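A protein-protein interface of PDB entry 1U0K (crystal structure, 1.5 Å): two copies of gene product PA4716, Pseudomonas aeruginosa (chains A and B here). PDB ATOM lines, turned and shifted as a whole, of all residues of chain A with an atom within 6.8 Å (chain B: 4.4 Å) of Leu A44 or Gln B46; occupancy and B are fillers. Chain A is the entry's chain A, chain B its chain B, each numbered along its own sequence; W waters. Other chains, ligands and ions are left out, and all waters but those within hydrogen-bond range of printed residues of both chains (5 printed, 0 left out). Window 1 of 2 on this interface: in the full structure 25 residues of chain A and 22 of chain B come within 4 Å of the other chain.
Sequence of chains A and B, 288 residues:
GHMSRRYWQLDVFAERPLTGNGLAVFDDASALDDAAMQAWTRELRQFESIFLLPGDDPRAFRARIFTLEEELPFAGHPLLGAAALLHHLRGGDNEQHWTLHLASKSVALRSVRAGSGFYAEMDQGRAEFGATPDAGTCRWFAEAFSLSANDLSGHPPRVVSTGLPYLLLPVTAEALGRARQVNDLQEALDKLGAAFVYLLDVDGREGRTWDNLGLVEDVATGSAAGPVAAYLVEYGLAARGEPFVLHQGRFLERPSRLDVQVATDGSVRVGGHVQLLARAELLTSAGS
The side-chain carboxylate of Glu A43 sits at hydrogen-bond distance from the side-chain amide nitrogen of Gln B9, 2.9 Å away.
The side-chain amide nitrogen (NE2) of Gln B46 sits at hydrogen-bond distance from the backbone carbonyl oxygen (O) of Glu A43.
The backbone carbonyl oxygen (O) of Leu A44 sits at hydrogen-bond distance from the side-chain amide nitrogen (NE2) of Gln B46, 3.5 Å away.
The guanidinium group (NE) of Arg A45 is in hydrogen-bond range of the backbone carbonyl oxygen (O) of Arg B45, 2.8 Å away.
NE2 of Gln A46 is in hydrogen-bond range of O of Leu B44 (3.3 Å).
O of Leu A44 sits close to O of Leu B44.
The side-chain amide oxygen (OE1) of Gln A46 is in hydrogen-bond range of the side-chain amide nitrogen (NE2) of Gln A9, 3.1 Å away.
NE2 of Gln A46 sits at hydrogen-bond distance from O of Leu A44.
The side-chain amide oxygen of Gln B9 sits close to the backbone carbonyl oxygen of Leu B23, 3.5 Å away.
The side-chain amide nitrogen of Gln B9 is in hydrogen-bond range of the side-chain amide oxygen of Gln B46 (3.1 Å).
O of Gly B22 lies close to OE1 of Gln B46, at 3.3 Å.
N of Leu B23 is in hydrogen-bond range of OE1 of Gln B46, at 3.4 Å.
Among the printed residues, merely in contact across the chains: Gln A46 with Arg B45, Arg A45 with Gln B46 and Arg A45 with Phe B47.
Leu A44 touches just these residues of chain B: Leu B44 (3.4 Å) and Gln B46 (3.5 Å).
Printed residues of chain B within 4 Å of Arg A45: Arg B45, Gln B46 and Phe B47.
Ala B24 touches none of the printed residues of chain A.
Of the printed residues of chain A, Gln B46 touches Glu A43 (3.0 Å), Leu A44 (3.5 Å) and Arg A45 (3.8 Å).
Of the printed residues of chain A, Phe B47 touches Arg A45.
The nearest printed residue of chain B that does not touch Leu A44 is Arg B45 (4.7 Å).
The nearest printed residue of chain A that does not touch Phe B47 is Glu A43 (7.6 Å).
Of the 18 printed residues of chain A, 4 touch a printed residue of chain B.
Among the printed residues, 9 pairs touch across the chains.
Among the printed residues, no Asp or Glu carboxylate lies within 4 Å of a Lys or Arg side-chain nitrogen of the other chain.
Leu A44 touches Gln B46, and with the chains exchanged Gln A46 touches Leu B44.
Arg A45 touches its own counterpart, Arg B45.
Arg A45 touches Gln B46, and with the chains exchanged Gln A46 touches Arg B45.
Arg A45 touches Phe B47, but with the chains exchanged Phe A47 does not touch Arg B45 (4.1 Å).
Of the 9 pairs that touch across the chains among the printed residues, 6 have their exchanged pair printed and touching as well.
Water W4 bridges O of Glu A43 (2.6 Å) and OE1 of Gln B46 (2.8 Å).
Water W1 lies within hydrogen-bond range of O of Leu B44 (2.7 Å), O of Leu A44 (2.7 Å) and NE2 of Gln B46 (3.3 Å).
Water W2 lies within hydrogen-bond range of the backbone carbonyl oxygen of Arg B45 and the guanidinium group of Arg A45.
Water W5 lies within hydrogen-bond range of the backbone carbonyl oxygen of Arg A45 (2.8 Å) and the guanidinium group of Arg B45 (3.2 Å).
Water W3 lies within hydrogen-bond range of the backbone NH of Phe A47, the guanidinium group of Arg B45 and the side-chain amide oxygen of Gln A46.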
ATOM      1  N   TYR A   7      13.139  15.036 -25.618  1.00  0.00           N
ATOM      2  CA  TYR A   7      12.877  13.829 -24.861  1.00  0.00           C
ATOM      3  C   TYR A   7      13.764  13.803 -23.630  1.00  0.00           C
ATOM      4  O   TYR A   7      14.715  14.598 -23.499  1.00  0.00           O
ATOM      5  CB  TYR A   7      13.028  12.569 -25.718  1.00  0.00           C
ATOM      6  CG  TYR A   7      14.440  12.232 -26.119  1.00  0.00           C
ATOM      7  CD1 TYR A   7      15.276  11.554 -25.265  1.00  0.00           C
ATOM      8  CD2 TYR A   7      14.934  12.624 -27.354  1.00  0.00           C
ATOM      9  CE1 TYR A   7      16.586  11.242 -25.632  1.00  0.00           C
ATOM     10  CE2 TYR A   7      16.243  12.306 -27.740  1.00  0.00           C
ATOM     11  CZ  TYR A   7      17.058  11.631 -26.865  1.00  0.00           C
ATOM     12  OH  TYR A   7      18.360  11.327 -27.207  1.00  0.00           O
ATOM     13  N   TRP A   8      13.439  12.915 -22.712  1.00  0.00           N
ATOM     14  CA  TRP A   8      14.124  12.823 -21.434  1.00  0.00           C
ATOM     15  C   TRP A   8      14.456  11.386 -21.129  1.00  0.00           C
ATOM     16  O   TRP A   8      13.630  10.515 -21.351  1.00  0.00           O
ATOM     17  CB  TRP A   8      13.250  13.371 -20.311  1.00  0.00           C
ATOM     18  CG  TRP A   8      12.700  14.735 -20.564  1.00  0.00           C
ATOM     19  CD1 TRP A   8      11.720  15.088 -21.463  1.00  0.00           C
ATOM     20  CD2 TRP A   8      13.069  15.946 -19.893  1.00  0.00           C
ATOM     21  NE1 TRP A   8      11.476  16.435 -21.390  1.00  0.00           N
ATOM     22  CE2 TRP A   8      12.285  16.983 -20.434  1.00  0.00           C
ATOM     23  CE3 TRP A   8      13.990  16.258 -18.880  1.00  0.00           C
ATOM     24  CZ2 TRP A   8      12.394  18.310 -20.000  1.00  0.00           C
ATOM     25  CZ3 TRP A   8      14.091  17.568 -18.458  1.00  0.00           C
ATOM     26  CH2 TRP A   8      13.296  18.570 -19.010  1.00  0.00           C
ATOM     27  N   GLN A   9      15.643  11.151 -20.580  1.00  0.00           N
ATOM     28  CA  GLN A   9      16.078   9.842 -20.129  1.00  0.00           C
ATOM     29  C   GLN A   9      15.887   9.771 -18.625  1.00  0.00           C
ATOM     30  O   GLN A   9      16.388  10.606 -17.896  1.00  0.00           O
ATOM     31  CB  GLN A   9      17.556   9.612 -20.499  1.00  0.00           C
ATOM     32  CG  GLN A   9      18.138   8.301 -20.012  1.00  0.00           C
ATOM     33  CD  GLN A   9      17.497   7.078 -20.637  1.00  0.00           C
ATOM     34  OE1 GLN A   9      16.904   7.157 -21.717  1.00  0.00           O
ATOM     35  NE2 GLN A   9      17.605   5.945 -19.954  1.00  0.00           N
ATOM     36  N   ALA A  24      12.701   6.389 -21.974  1.00  0.00           N
ATOM     37  CA  ALA A  24      12.643   7.681 -22.650  1.00  0.00           C
ATOM     38  C   ALA A  24      11.218   8.224 -22.626  1.00  0.00           C
ATOM     39  O   ALA A  24      10.264   7.487 -22.874  1.00  0.00           O
ATOM     40  CB  ALA A  24      13.131   7.592 -24.067  1.00  0.00           C
ATOM     41  N   VAL A  25      11.085   9.512 -22.315  1.00  0.00           N
ATOM     42  CA  VAL A  25       9.795  10.189 -22.266  1.00  0.00           C
ATOM     43  C   VAL A  25       9.816  11.395 -23.186  1.00  0.00           C
ATOM     44  O   VAL A  25      10.697  12.230 -23.071  1.00  0.00           O
ATOM     45  CB  VAL A  25       9.481  10.692 -20.844  1.00  0.00           C
ATOM     46  CG1 VAL A  25       8.112  11.399 -20.799  1.00  0.00           C
ATOM     47  CG2 VAL A  25       9.540   9.562 -19.829  1.00  0.00           C
ATOM     48  N   PHE A  26       8.857  11.476 -24.097  1.00  0.00           N
ATOM     49  CA  PHE A  26       8.678  12.625 -24.976  1.00  0.00           C
ATOM     50  C   PHE A  26       7.503  13.402 -24.376  1.00  0.00           C
ATOM     51  O   PHE A  26       6.377  12.938 -24.405  1.00  0.00           O
ATOM     52  CB  PHE A  26       8.382  12.175 -26.414  1.00  0.00           C
ATOM     53  CG  PHE A  26       9.552  11.543 -27.127  1.00  0.00           C
ATOM     54  CD1 PHE A  26      10.049  10.314 -26.732  1.00  0.00           C
ATOM     55  CD2 PHE A  26      10.145  12.185 -28.218  1.00  0.00           C
ATOM     56  CE1 PHE A  26      11.128   9.729 -27.407  1.00  0.00           C
ATOM     57  CE2 PHE A  26      11.198  11.593 -28.896  1.00  0.00           C
ATOM     58  CZ  PHE A  26      11.688  10.389 -28.489  1.00  0.00           C
ATOM     59  N   ALA A  39       9.620   4.641 -34.639  1.00  0.00           N
ATOM     60  CA  ALA A  39      10.989   4.834 -35.115  1.00  0.00           C
ATOM     61  C   ALA A  39      11.864   5.464 -34.025  1.00  0.00           C
ATOM     62  O   ALA A  39      13.018   5.080 -33.874  1.00  0.00           O
ATOM     63  CB  ALA A  39      11.017   5.659 -36.383  1.00  0.00           C
ATOM     64  N   TRP A  40      11.320   6.425 -33.277  1.00  0.00           N
ATOM     65  CA  TRP A  40      12.056   7.058 -32.168  1.00  0.00           C
ATOM     66  C   TRP A  40      12.289   6.060 -31.044  1.00  0.00           C
ATOM     67  O   TRP A  40      13.329   6.091 -30.385  1.00  0.00           O
ATOM     68  CB  TRP A  40      11.324   8.306 -31.636  1.00  0.00           C
ATOM     69  CG  TRP A  40      11.739   9.557 -32.289  1.00  0.00           C
ATOM     70  CD1 TRP A  40      11.029  10.297 -33.179  1.00  0.00           C
ATOM     71  CD2 TRP A  40      13.001  10.204 -32.149  1.00  0.00           C
ATOM     72  NE1 TRP A  40      11.759  11.393 -33.573  1.00  0.00           N
ATOM     73  CE2 TRP A  40      12.979  11.353 -32.956  1.00  0.00           C
ATOM     74  CE3 TRP A  40      14.147   9.943 -31.392  1.00  0.00           C
ATOM     75  CZ2 TRP A  40      14.063  12.232 -33.036  1.00  0.00           C
ATOM     76  CZ3 TRP A  40      15.225  10.812 -31.483  1.00  0.00           C
ATOM     77  CH2 TRP A  40      15.173  11.936 -32.296  1.00  0.00           C
ATOM     78  N   THR A  41      11.340   5.160 -30.813  1.00  0.00           N
ATOM     79  CA  THR A  41      11.509   4.124 -29.794  1.00  0.00           C
ATOM     80  C   THR A  41      12.713   3.247 -30.165  1.00  0.00           C
ATOM     81  O   THR A  41      13.546   2.918 -29.316  1.00  0.00           O
ATOM     82  CB  THR A  41      10.213   3.302 -29.680  1.00  0.00           C
ATOM     83  OG1 THR A  41       9.137   4.163 -29.260  1.00  0.00           O
ATOM     84  CG2 THR A  41      10.323   2.258 -28.576  1.00  0.00           C
ATOM     85  N   ARG A  42      12.808   2.880 -31.438  1.00  0.00           N
ATOM     86  CA  ARG A  42      13.924   2.072 -31.934  1.00  0.00           C
ATOM     87  C   ARG A  42      15.232   2.855 -31.905  1.00  0.00           C
ATOM     88  O   ARG A  42      16.303   2.278 -31.686  1.00  0.00           O
ATOM     89  CB  ARG A  42      13.616   1.551 -33.332  1.00  0.00           C
ATOM     90  CG  ARG A  42      12.617   0.425 -33.294  1.00  0.00           C
ATOM     91  CD  ARG A  42      11.951   0.130 -34.617  1.00  0.00           C
ATOM     92  NE  ARG A  42      10.973  -0.933 -34.422  1.00  0.00           N
ATOM     93  CZ  ARG A  42      10.062  -1.304 -35.315  1.00  0.00           C
ATOM     94  NH1 ARG A  42       9.988  -0.708 -36.496  1.00  0.00           N
ATOM     95  NH2 ARG A  42       9.220  -2.284 -35.022  1.00  0.00           N
ATOM     96  N   GLU A  43      15.150   4.163 -32.108  1.00  0.00           N
ATOM     97  CA  GLU A  43      16.325   5.031 -32.023  1.00  0.00           C
ATOM     98  C   GLU A  43      16.929   5.013 -30.618  1.00  0.00           C
ATOM     99  O   GLU A  43      18.139   4.833 -30.466  1.00  0.00           O
ATOM    100  CB  GLU A  43      15.951   6.464 -32.386  1.00  0.00           C
ATOM    101  CG  GLU A  43      17.119   7.427 -32.468  1.00  0.00           C
ATOM    102  CD  GLU A  43      18.030   7.162 -33.635  1.00  0.00           C
ATOM    103  OE1 GLU A  43      19.185   7.610 -33.574  1.00  0.00           O
ATOM    104  OE2 GLU A  43      17.593   6.548 -34.640  1.00  0.00           O
ATOM    105  N   LEU A  44      16.097   5.187 -29.601  1.00  0.00           N
ATOM    106  CA  LEU A  44      16.600   5.376 -28.250  1.00  0.00           C
ATOM    107  C   LEU A  44      16.913   4.068 -27.531  1.00  0.00           C
ATOM    108  O   LEU A  44      17.667   4.069 -26.562  1.00  0.00           O
ATOM    109  CB  LEU A  44      15.629   6.237 -27.451  1.00  0.00           C
ATOM    110  CG  LEU A  44      15.445   7.645 -28.023  1.00  0.00           C
ATOM    111  CD1 LEU A  44      14.582   8.483 -27.102  1.00  0.00           C
ATOM    112  CD2 LEU A  44      16.804   8.317 -28.294  1.00  0.00           C
ATOM    113  N   ARG A  45      16.343   2.954 -28.000  1.00  0.00           N
ATOM    114  CA  ARG A  45      16.669   1.594 -27.541  1.00  0.00           C
ATOM    115  C   ARG A  45      16.394   1.307 -26.067  1.00  0.00           C
ATOM    116  O   ARG A  45      16.854   0.300 -25.525  1.00  0.00           O
ATOM    117  CB  ARG A  45      18.108   1.234 -27.930  1.00  0.00           C
ATOM    118  CG  ARG A  45      18.298   1.276 -29.422  1.00  0.00           C
ATOM    119  CD  ARG A  45      19.729   1.234 -29.836  1.00  0.00           C
ATOM    120  NE  ARG A  45      20.359  -0.030 -29.488  1.00  0.00           N
ATOM    121  CZ  ARG A  45      20.411  -1.094 -30.269  1.00  0.00           C
ATOM    122  NH1 ARG A  45      19.821  -1.083 -31.454  1.00  0.00           N
ATOM    123  NH2 ARG A  45      21.054  -2.184 -29.856  1.00  0.00           N
ATOM    124  N   GLN A  46      15.613   2.165 -25.420  1.00  0.00           N
ATOM    125  CA  GLN A  46      15.095   1.846 -24.107  1.00  0.00           C
ATOM    126  C   GLN A  46      14.005   0.787 -24.284  1.00  0.00           C
ATOM    127  O   GLN A  46      13.361   0.748 -25.335  1.00  0.00           O
ATOM    128  CB  GLN A  46      14.556   3.114 -23.440  1.00  0.00           C
ATOM    129  CG  GLN A  46      15.594   4.219 -23.375  1.00  0.00           C
ATOM    130  CD  GLN A  46      16.824   3.812 -22.570  1.00  0.00           C
ATOM    131  OE1 GLN A  46      16.701   3.411 -21.416  1.00  0.00           O
ATOM    132  NE2 GLN A  46      18.011   3.906 -23.184  1.00  0.00           N
ATOM    133  N   PHE A  47      13.828  -0.071 -23.298  1.00  0.00           N
ATOM    134  CA  PHE A  47      12.896  -1.198 -23.423  1.00  0.00           C
ATOM    135  C   PHE A  47      11.512  -0.660 -23.812  1.00  0.00           C
ATOM    136  O   PHE A  47      10.825  -1.254 -24.635  1.00  0.00           O
ATOM    137  CB  PHE A  47      12.834  -2.031 -22.143  1.00  0.00           C
ATOM    138  CG  PHE A  47      12.258  -3.417 -22.338  1.00  0.00           C
ATOM    139  CD1 PHE A  47      13.092  -4.521 -22.528  1.00  0.00           C
ATOM    140  CD2 PHE A  47      10.887  -3.619 -22.331  1.00  0.00           C
ATOM    141  CE1 PHE A  47      12.558  -5.803 -22.701  1.00  0.00           C
ATOM    142  CE2 PHE A  47      10.351  -4.901 -22.516  1.00  0.00           C
ATOM    143  CZ  PHE A  47      11.184  -5.982 -22.701  1.00  0.00           C
ATOM    144  N   SER A  49       9.608   3.365 -24.692  1.00  0.00           N
ATOM    145  CA  SER A  49       9.491   4.827 -24.725  1.00  0.00           C
ATOM    146  C   SER A  49       8.013   5.189 -24.568  1.00  0.00           C
ATOM    147  O   SER A  49       7.136   4.444 -24.992  1.00  0.00           O
ATOM    148  CB  SER A  49      10.022   5.428 -26.027  1.00  0.00           C
ATOM    149  OG  SER A  49      11.440   5.354 -26.119  1.00  0.00           O
ATOM    150  N   PHE A  51       5.197   8.506 -25.061  1.00  0.00           N
ATOM    151  CA  PHE A  51       4.948   9.738 -25.808  1.00  0.00           C
ATOM    152  C   PHE A  51       3.699  10.382 -25.233  1.00  0.00           C
ATOM    153  O   PHE A  51       2.656   9.740 -25.180  1.00  0.00           O
ATOM    154  CB  PHE A  51       4.764   9.418 -27.298  1.00  0.00           C
ATOM    155  CG  PHE A  51       5.982   8.799 -27.927  1.00  0.00           C
ATOM    156  CD1 PHE A  51       6.203   7.432 -27.817  1.00  0.00           C
ATOM    157  CD2 PHE A  51       6.926   9.576 -28.589  1.00  0.00           C
ATOM    158  CE1 PHE A  51       7.340   6.859 -28.343  1.00  0.00           C
ATOM    159  CE2 PHE A  51       8.075   8.995 -29.108  1.00  0.00           C
ATOM    160  CZ  PHE A  51       8.271   7.633 -28.986  1.00  0.00           C
ATOM    161  N   LEU A  68      10.365  -1.854 -28.637  1.00  0.00           N
ATOM    162  CA  LEU A  68      11.026  -1.881 -29.929  1.00  0.00           C
ATOM    163  C   LEU A  68      10.254  -2.749 -30.919  1.00  0.00           C
ATOM    164  O   LEU A  68      10.473  -2.640 -32.118  1.00  0.00           O
ATOM    165  CB  LEU A  68      12.485  -2.345 -29.806  1.00  0.00           C
ATOM    166  CG  LEU A  68      13.442  -1.170 -29.605  1.00  0.00           C
ATOM    167  CD1 LEU A  68      13.381  -0.644 -28.195  1.00  0.00           C
ATOM    168  CD2 LEU A  68      14.865  -1.543 -29.961  1.00  0.00           C
ATOM    169  N   GLN B   9      23.166  12.339 -29.895  1.00  0.00           N
ATOM    170  CA  GLN B   9      22.639  11.164 -30.580  1.00  0.00           C
ATOM    171  C   GLN B   9      22.780  11.355 -32.093  1.00  0.00           C
ATOM    172  O   GLN B   9      22.277  12.334 -32.640  1.00  0.00           O
ATOM    173  CB  GLN B   9      21.172  10.971 -30.229  1.00  0.00           C
ATOM    174  CG  GLN B   9      20.543   9.734 -30.874  1.00  0.00           C
ATOM    175  CD  GLN B   9      21.116   8.400 -30.396  1.00  0.00           C
ATOM    176  OE1 GLN B   9      21.742   8.308 -29.339  1.00  0.00           O
ATOM    177  NE2 GLN B   9      20.891   7.355 -31.189  1.00  0.00           N
ATOM    178  N   GLY B  22      22.452   3.883 -34.658  1.00  0.00           N
ATOM    179  CA  GLY B  22      22.383   4.908 -33.637  1.00  0.00           C
ATOM    180  C   GLY B  22      23.607   4.851 -32.741  1.00  0.00           C
ATOM    181  O   GLY B  22      24.120   3.787 -32.428  1.00  0.00           O
ATOM    182  N   LEU B  23      24.039   6.020 -32.309  1.00  0.00           N
ATOM    183  CA  LEU B  23      25.316   6.192 -31.616  1.00  0.00           C
ATOM    184  C   LEU B  23      25.220   7.374 -30.660  1.00  0.00           C
ATOM    185  O   LEU B  23      24.758   8.429 -31.053  1.00  0.00           O
ATOM    186  CB  LEU B  23      26.411   6.478 -32.640  1.00  0.00           C
ATOM    187  CG  LEU B  23      27.799   6.862 -32.126  1.00  0.00           C
ATOM    188  CD1 LEU B  23      28.542   5.646 -31.607  1.00  0.00           C
ATOM    189  CD2 LEU B  23      28.593   7.573 -33.216  1.00  0.00           C
ATOM    190  N   ALA B  24      25.683   7.206 -29.425  1.00  0.00           N
ATOM    191  CA  ALA B  24      25.860   8.330 -28.500  1.00  0.00           C
ATOM    192  C   ALA B  24      27.325   8.744 -28.508  1.00  0.00           C
ATOM    193  O   ALA B  24      28.199   7.893 -28.453  1.00  0.00           O
ATOM    194  CB  ALA B  24      25.434   7.941 -27.110  1.00  0.00           C
ATOM    195  N   LEU B  44      22.407   4.144 -21.959  1.00  0.00           N
ATOM    196  CA  LEU B  44      21.868   4.658 -23.219  1.00  0.00           C
ATOM    197  C   LEU B  44      21.498   3.560 -24.207  1.00  0.00           C
ATOM    198  O   LEU B  44      20.712   3.789 -25.109  1.00  0.00           O
ATOM    199  CB  LEU B  44      22.847   5.657 -23.850  1.00  0.00           C
ATOM    200  CG  LEU B  44      23.136   6.888 -22.986  1.00  0.00           C
ATOM    201  CD1 LEU B  44      24.104   7.795 -23.712  1.00  0.00           C
ATOM    202  CD2 LEU B  44      21.862   7.642 -22.630  1.00  0.00           C
ATOM    203  N   ARG B  45      22.082   2.376 -24.040  1.00  0.00           N
ATOM    204  CA  ARG B  45      21.724   1.180 -24.791  1.00  0.00           C
ATOM    205  C   ARG B  45      21.976   1.236 -26.296  1.00  0.00           C
ATOM    206  O   ARG B  45      21.511   0.366 -27.021  1.00  0.00           O
ATOM    207  CB  ARG B  45      20.266   0.778 -24.512  1.00  0.00           C
ATOM    208  CG  ARG B  45      20.031   0.374 -23.080  1.00  0.00           C
ATOM    209  CD  ARG B  45      18.587   0.368 -22.677  1.00  0.00           C
ATOM    210  NE  ARG B  45      17.893  -0.827 -23.130  1.00  0.00           N
ATOM    211  CZ  ARG B  45      17.594  -1.874 -22.358  1.00  0.00           C
ATOM    212  NH1 ARG B  45      17.965  -1.919 -21.079  1.00  0.00           N
ATOM    213  NH2 ARG B  45      16.933  -2.897 -22.881  1.00  0.00           N
ATOM    214  N   GLN B  46      22.715   2.232 -26.777  1.00  0.00           N
ATOM    215  CA  GLN B  46      23.203   2.225 -28.156  1.00  0.00           C
ATOM    216  C   GLN B  46      24.212   1.098 -28.258  1.00  0.00           C
ATOM    217  O   GLN B  46      24.902   0.789 -27.279  1.00  0.00           O
ATOM    218  CB  GLN B  46      23.826   3.580 -28.520  1.00  0.00           C
ATOM    219  CG  GLN B  46      22.864   4.734 -28.319  1.00  0.00           C
ATOM    220  CD  GLN B  46      21.621   4.631 -29.161  1.00  0.00           C
ATOM    221  OE1 GLN B  46      21.693   4.472 -30.376  1.00  0.00           O
ATOM    222  NE2 GLN B  46      20.466   4.700 -28.504  1.00  0.00           N
ATOM    223  N   PHE B  47      24.282   0.440 -29.405  1.00  0.00           N
ATOM    224  CA  PHE B  47      25.119  -0.765 -29.506  1.00  0.00           C
ATOM    225  C   PHE B  47      26.549  -0.405 -29.103  1.00  0.00           C
ATOM    226  O   PHE B  47      27.207  -1.160 -28.362  1.00  0.00           O
ATOM    227  CB  PHE B  47      25.053  -1.381 -30.905  1.00  0.00           C
ATOM    228  CG  PHE B  47      25.583  -2.785 -30.987  1.00  0.00           C
ATOM    229  CD1 PHE B  47      24.719  -3.860 -30.921  1.00  0.00           C
ATOM    230  CD2 PHE B  47      26.942  -3.035 -31.140  1.00  0.00           C
ATOM    231  CE1 PHE B  47      25.193  -5.170 -30.994  1.00  0.00           C
ATOM    232  CE2 PHE B  47      27.413  -4.339 -31.218  1.00  0.00           C
ATOM    233  CZ  PHE B  47      26.545  -5.398 -31.128  1.00  0.00           C
ATOM    234  N   GLU B  48      26.989   0.759 -29.553  1.00  0.00           N
ATOM    235  CA  GLU B  48      28.219   1.395 -29.067  1.00  0.00           C
ATOM    236  C   GLU B  48      27.998   2.851 -28.700  1.00  0.00           C
ATOM    237  O   GLU B  48      27.151   3.525 -29.280  1.00  0.00           O
ATOM    238  CB  GLU B  48      29.320   1.304 -30.115  1.00  0.00           C
ATOM    239  CG  GLU B  48      29.939  -0.086 -30.151  1.00  0.00           C
ATOM    240  CD  GLU B  48      30.552  -0.473 -31.473  1.00  0.00           C
ATOM    241  OE1 GLU B  48      31.097   0.375 -32.191  1.00  0.00           O
ATOM    242  OE2 GLU B  48      30.505  -1.689 -31.778  1.00  0.00           O
ATOM    243  N   SER B  49      28.745   3.309 -27.700  1.00  0.00           N
ATOM    244  CA  SER B  49      28.882   4.732 -27.399  1.00  0.00           C
ATOM    245  C   SER B  49      30.382   5.056 -27.529  1.00  0.00           C
ATOM    246  O   SER B  49      31.244   4.188 -27.352  1.00  0.00           O
ATOM    247  CB  SER B  49      28.356   5.085 -25.999  1.00  0.00           C
ATOM    248  OG  SER B  49      26.916   5.094 -25.946  1.00  0.00           O
ATOM    249  N   LEU B  68      27.952  -2.657 -24.778  1.00  0.00           N
ATOM    250  CA  LEU B  68      27.398  -2.921 -23.459  1.00  0.00           C
ATOM    251  C   LEU B  68      28.207  -3.984 -22.703  1.00  0.00           C
ATOM    252  O   LEU B  68      28.123  -4.062 -21.497  1.00  0.00           O
ATOM    253  CB  LEU B  68      25.899  -3.290 -23.544  1.00  0.00           C
ATOM    254  CG  LEU B  68      24.985  -2.055 -23.497  1.00  0.00           C
ATOM    255  CD1 LEU B  68      25.008  -1.264 -24.789  1.00  0.00           C
ATOM    256  CD2 LEU B  68      23.570  -2.440 -23.170  1.00  0.00           C
HETATM  257  O   HOH W   1      19.338   5.984 -25.684  1.00  0.00           O
HETATM  258  O   HOH W   2      21.701  -2.436 -27.004  1.00  0.00           O
HETATM  259  O   HOH W   3      15.335   0.285 -20.850  1.00  0.00           O
HETATM  260  O   HOH W   4      19.718   3.478 -32.090  1.00  0.00           O
HETATM  261  O   HOH W   5      16.747  -2.475 -26.024  1.00  0.00           O
